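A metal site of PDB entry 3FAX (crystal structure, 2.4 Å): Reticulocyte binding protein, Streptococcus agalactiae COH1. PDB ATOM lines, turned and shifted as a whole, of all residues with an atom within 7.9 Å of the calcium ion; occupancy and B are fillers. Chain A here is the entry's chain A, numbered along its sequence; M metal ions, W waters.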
ATOM      1  N   ASP A 164     -11.679  -8.890  -1.443  1.00  0.00           N
ATOM      2  CA  ASP A 164     -12.314 -10.210  -1.439  1.00  0.00           C
ATOM      3  C   ASP A 164     -11.353 -11.279  -0.951  1.00  0.00           C
ATOM      4  O   ASP A 164     -10.202 -11.346  -1.399  1.00  0.00           O
ATOM      5  CB  ASP A 164     -12.836 -10.560  -2.837  1.00  0.00           C
ATOM      6  CG  ASP A 164     -13.794 -11.750  -2.836  1.00  0.00           C
ATOM      7  OD1 ASP A 164     -13.768 -12.558  -1.895  1.00  0.00           O
ATOM      8  OD2 ASP A 164     -14.586 -11.863  -3.794  1.00  0.00           O
ATOM      9  N   LYS A 165     -11.841 -12.124  -0.038  1.00  0.00           N
ATOM     10  CA  LYS A 165     -11.071 -13.272   0.463  1.00  0.00           C
ATOM     11  C   LYS A 165     -10.668 -14.255  -0.636  1.00  0.00           C
ATOM     12  O   LYS A 165      -9.579 -14.838  -0.594  1.00  0.00           O
ATOM     13  CB  LYS A 165     -11.869 -14.021   1.550  1.00  0.00           C
ATOM     14  CG  LYS A 165     -13.200 -14.617   1.091  1.00  0.00           C
ATOM     15  CD  LYS A 165     -13.894 -15.336   2.242  1.00  0.00           C
ATOM     16  CE  LYS A 165     -15.361 -15.618   1.948  1.00  0.00           C
ATOM     17  NZ  LYS A 165     -16.002 -16.424   3.025  1.00  0.00           N
ATOM     18  N   ASP A 166     -11.560 -14.420  -1.610  1.00  0.00           N
ATOM     19  CA  ASP A 166     -11.340 -15.348  -2.723  1.00  0.00           C
ATOM     20  C   ASP A 166     -10.708 -14.663  -3.936  1.00  0.00           C
ATOM     21  O   ASP A 166     -10.449 -15.317  -4.952  1.00  0.00           O
ATOM     22  CB  ASP A 166     -12.675 -16.026  -3.093  1.00  0.00           C
ATOM     23  CG  ASP A 166     -13.173 -16.973  -2.006  1.00  0.00           C
ATOM     24  OD1 ASP A 166     -12.367 -17.391  -1.144  1.00  0.00           O
ATOM     25  OD2 ASP A 166     -14.374 -17.323  -2.004  1.00  0.00           O
ATOM     26  N   ASN A 167     -10.468 -13.356  -3.840  1.00  0.00           N
ATOM     27  CA  ASN A 167      -9.758 -12.604  -4.870  1.00  0.00           C
ATOM     28  C   ASN A 167      -9.316 -11.252  -4.313  1.00  0.00           C
ATOM     29  O   ASN A 167     -10.097 -10.318  -4.234  1.00  0.00           O
ATOM     30  CB  ASN A 167     -10.655 -12.416  -6.097  1.00  0.00           C
ATOM     31  CG  ASN A 167     -10.077 -11.440  -7.118  1.00  0.00           C
ATOM     32  OD1 ASN A 167      -8.956 -10.934  -6.959  1.00  0.00           O
ATOM     33  ND2 ASN A 167     -10.843 -11.160  -8.164  1.00  0.00           N
ATOM     34  N   GLN A 168      -8.049 -11.162  -3.908  1.00  0.00           N
ATOM     35  CA  GLN A 168      -7.547 -10.012  -3.160  1.00  0.00           C
ATOM     36  C   GLN A 168      -7.525  -8.704  -3.948  1.00  0.00           C
ATOM     37  O   GLN A 168      -7.445  -7.629  -3.357  1.00  0.00           O
ATOM     38  CB  GLN A 168      -6.147 -10.296  -2.617  1.00  0.00           C
ATOM     39  CG  GLN A 168      -5.094 -10.557  -3.679  1.00  0.00           C
ATOM     40  CD  GLN A 168      -3.689 -10.560  -3.117  1.00  0.00           C
ATOM     41  OE1 GLN A 168      -3.019 -11.600  -3.104  1.00  0.00           O
ATOM     42  NE2 GLN A 168      -3.229  -9.403  -2.648  1.00  0.00           N
ATOM     43  N   THR A 199     -13.746 -13.412   8.314  1.00  0.00           N
ATOM     44  CA  THR A 199     -12.538 -14.232   8.379  1.00  0.00           C
ATOM     45  C   THR A 199     -12.008 -14.427   6.961  1.00  0.00           C
ATOM     46  O   THR A 199     -12.766 -14.703   6.037  1.00  0.00           O
ATOM     47  CB  THR A 199     -12.750 -15.632   9.059  1.00  0.00           C
ATOM     48  OG1 THR A 199     -13.681 -16.406   8.290  1.00  0.00           O
ATOM     49  CG2 THR A 199     -13.264 -15.480  10.482  1.00  0.00           C
ATOM     50  N   GLY A 200     -10.704 -14.237   6.790  1.00  0.00           N
ATOM     51  CA  GLY A 200     -10.077 -14.421   5.484  1.00  0.00           C
ATOM     52  C   GLY A 200     -10.165 -13.235   4.523  1.00  0.00           C
ATOM     53  O   GLY A 200      -9.486 -13.234   3.503  1.00  0.00           O
ATOM     54  N   TYR A 201     -10.996 -12.231   4.830  1.00  0.00           N
ATOM     55  CA  TYR A 201     -11.050 -11.019   3.996  1.00  0.00           C
ATOM     56  C   TYR A 201      -9.804 -10.184   4.240  1.00  0.00           C
ATOM     57  O   TYR A 201      -9.184 -10.282   5.298  1.00  0.00           O
ATOM     58  CB  TYR A 201     -12.336 -10.207   4.257  1.00  0.00           C
ATOM     59  CG  TYR A 201     -13.522 -10.718   3.482  1.00  0.00           C
ATOM     60  CD1 TYR A 201     -14.316 -11.752   3.990  1.00  0.00           C
ATOM     61  CD2 TYR A 201     -13.854 -10.196   2.223  1.00  0.00           C
ATOM     62  CE1 TYR A 201     -15.392 -12.244   3.287  1.00  0.00           C
ATOM     63  CE2 TYR A 201     -14.927 -10.686   1.506  1.00  0.00           C
ATOM     64  CZ  TYR A 201     -15.694 -11.718   2.038  1.00  0.00           C
ATOM     65  OH  TYR A 201     -16.761 -12.213   1.337  1.00  0.00           O
ATOM     66  N   TYR A 202      -9.424  -9.377   3.267  1.00  0.00           N
ATOM     67  CA  TYR A 202      -8.192  -8.621   3.359  1.00  0.00           C
ATOM     68  C   TYR A 202      -8.469  -7.146   3.461  1.00  0.00           C
ATOM     69  O   TYR A 202      -9.548  -6.687   3.094  1.00  0.00           O
ATOM     70  CB  TYR A 202      -7.290  -8.915   2.151  1.00  0.00           C
ATOM     71  CG  TYR A 202      -7.053 -10.389   1.940  1.00  0.00           C
ATOM     72  CD1 TYR A 202      -7.646 -11.063   0.883  1.00  0.00           C
ATOM     73  CD2 TYR A 202      -6.258 -11.122   2.804  1.00  0.00           C
ATOM     74  CE1 TYR A 202      -7.443 -12.414   0.677  1.00  0.00           C
ATOM     75  CE2 TYR A 202      -6.054 -12.486   2.618  1.00  0.00           C
ATOM     76  CZ  TYR A 202      -6.641 -13.121   1.547  1.00  0.00           C
ATOM     77  OH  TYR A 202      -6.444 -14.462   1.333  1.00  0.00           O
ATOM     78  N   LEU A 224      -1.672 -12.192   6.243  1.00  0.00           N
ATOM     79  CA  LEU A 224      -1.742 -11.441   4.981  1.00  0.00           C
ATOM     80  C   LEU A 224      -2.323 -12.269   3.832  1.00  0.00           C
ATOM     81  O   LEU A 224      -2.446 -13.501   3.903  1.00  0.00           O
ATOM     82  CB  LEU A 224      -0.363 -10.944   4.563  1.00  0.00           C
ATOM     83  CG  LEU A 224       0.558 -10.344   5.636  1.00  0.00           C
ATOM     84  CD1 LEU A 224       1.992 -10.311   5.138  1.00  0.00           C
ATOM     85  CD2 LEU A 224       0.082  -8.959   6.045  1.00  0.00           C
ATOM     86  N   ALA A 225      -2.679 -11.562   2.763  1.00  0.00           N
ATOM     87  CA  ALA A 225      -3.034 -12.209   1.510  1.00  0.00           C
ATOM     88  C   ALA A 225      -1.767 -12.813   0.936  1.00  0.00           C
ATOM     89  O   ALA A 225      -0.659 -12.414   1.318  1.00  0.00           O
ATOM     90  CB  ALA A 225      -3.631 -11.199   0.528  1.00  0.00           C
ATOM     91  N   GLU A 226      -1.902 -13.800   0.061  1.00  0.00           N
ATOM     92  CA  GLU A 226      -0.741 -14.306  -0.662  1.00  0.00           C
ATOM     93  C   GLU A 226      -0.012 -13.108  -1.302  1.00  0.00           C
ATOM     94  O   GLU A 226      -0.644 -12.233  -1.863  1.00  0.00           O
ATOM     95  CB  GLU A 226      -1.141 -15.382  -1.696  1.00  0.00           C
ATOM     96  CG  GLU A 226      -1.890 -14.883  -2.968  1.00  0.00           C
ATOM     97  CD  GLU A 226      -3.382 -14.583  -2.758  1.00  0.00           C
ATOM     98  OE1 GLU A 226      -3.993 -14.032  -3.704  1.00  0.00           O
ATOM     99  OE2 GLU A 226      -3.949 -14.892  -1.692  1.00  0.00           O
ATOM    100  N   LYS A 361      -0.793 -23.683   1.916  1.00  0.00           N
ATOM    101  CA  LYS A 361      -1.941 -22.930   1.394  1.00  0.00           C
ATOM    102  C   LYS A 361      -1.757 -21.434   1.640  1.00  0.00           C
ATOM    103  O   LYS A 361      -2.348 -20.892   2.571  1.00  0.00           O
ATOM    104  CB  LYS A 361      -3.232 -23.421   2.047  1.00  0.00           C
ATOM    105  CG  LYS A 361      -3.584 -24.853   1.733  1.00  0.00           C
ATOM    106  CD  LYS A 361      -5.068 -25.140   1.978  1.00  0.00           C
ATOM    107  CE  LYS A 361      -5.509 -26.463   1.366  1.00  0.00           C
ATOM    108  NZ  LYS A 361      -7.001 -26.576   1.295  1.00  0.00           N
ATOM    109  N   PRO A 362      -0.937 -20.753   0.824  1.00  0.00           N
ATOM    110  CA  PRO A 362      -0.643 -19.319   1.017  1.00  0.00           C
ATOM    111  C   PRO A 362      -1.821 -18.377   0.765  1.00  0.00           C
ATOM    112  O   PRO A 362      -1.808 -17.235   1.229  1.00  0.00           O
ATOM    113  CB  PRO A 362       0.475 -19.036   0.009  1.00  0.00           C
ATOM    114  CG  PRO A 362       0.339 -20.096  -1.021  1.00  0.00           C
ATOM    115  CD  PRO A 362      -0.149 -21.318  -0.292  1.00  0.00           C
ATOM    116  N   LYS A 363      -2.825 -18.841   0.021  1.00  0.00           N
ATOM    117  CA  LYS A 363      -4.048 -18.076  -0.200  1.00  0.00           C
ATOM    118  C   LYS A 363      -4.980 -18.085   1.014  1.00  0.00           C
ATOM    119  O   LYS A 363      -5.819 -17.182   1.160  1.00  0.00           O
ATOM    120  CB  LYS A 363      -4.793 -18.636  -1.416  1.00  0.00           C
ATOM    121  CG  LYS A 363      -4.138 -18.375  -2.748  1.00  0.00           C
ATOM    122  CD  LYS A 363      -4.903 -19.110  -3.851  1.00  0.00           C
ATOM    123  CE  LYS A 363      -4.797 -18.409  -5.199  1.00  0.00           C
ATOM    124  NZ  LYS A 363      -5.630 -19.100  -6.224  1.00  0.00           N
ATOM    125  N   ASP A 364      -4.862 -19.106   1.856  1.00  0.00           N
ATOM    126  CA  ASP A 364      -5.567 -19.178   3.125  1.00  0.00           C
ATOM    127  C   ASP A 364      -4.717 -18.517   4.217  1.00  0.00           C
ATOM    128  O   ASP A 364      -3.722 -19.102   4.664  1.00  0.00           O
ATOM    129  CB  ASP A 364      -5.840 -20.648   3.492  1.00  0.00           C
ATOM    130  CG  ASP A 364      -6.628 -20.811   4.795  1.00  0.00           C
ATOM    131  OD1 ASP A 364      -6.880 -19.808   5.501  1.00  0.00           O
ATOM    132  OD2 ASP A 364      -7.004 -21.963   5.098  1.00  0.00           O
ATOM    133  N   PRO A 365      -5.092 -17.296   4.649  1.00  0.00           N
ATOM    134  CA  PRO A 365      -4.256 -16.555   5.595  1.00  0.00           C
ATOM    135  C   PRO A 365      -4.221 -17.188   6.995  1.00  0.00           C
ATOM    136  O   PRO A 365      -3.307 -16.909   7.763  1.00  0.00           O
ATOM    137  CB  PRO A 365      -4.936 -15.182   5.652  1.00  0.00           C
ATOM    138  CG  PRO A 365      -6.350 -15.457   5.329  1.00  0.00           C
ATOM    139  CD  PRO A 365      -6.384 -16.645   4.419  1.00  0.00           C
ATOM    140  N   SER A 366      -5.205 -18.026   7.303  1.00  0.00           N
ATOM    141  CA  SER A 366      -5.208 -18.760   8.578  1.00  0.00           C
ATOM    142  C   SER A 366      -4.177 -19.910   8.594  1.00  0.00           C
ATOM    143  O   SER A 366      -3.723 -20.328   9.667  1.00  0.00           O
ATOM    144  CB  SER A 366      -6.614 -19.307   8.897  1.00  0.00           C
ATOM    145  OG  SER A 366      -7.509 -18.272   9.243  1.00  0.00           O
HETATM  146 CA    CA M   1      -8.012 -16.587   0.577  1.00  0.00          CA
HETATM  147  O   HOH W   1      -8.296 -17.671  -1.440  1.00  0.00           O
HETATM  148  O   HOH W   2      -7.047 -15.128  -1.077  1.00  0.00           O
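Of the 18 residues printed, 3 come within 4 Å of the calcium ion.
The nearest printed residue that does not touch the calcium ion is Pro 365 (4.2 Å).
Water W1 binds the calcium ion, 2.3 Å away.
The calcium ion is bound by the backbone carbonyl oxygen (O) of Lys 363.
The calcium ion is bound by water W2 (2.4 Å).
The calcium ion is bound by the backbone carbonyl oxygen (O) of Lys 165.
The calcium ion is bound by OH of Tyr 202, at 2.7 Å.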
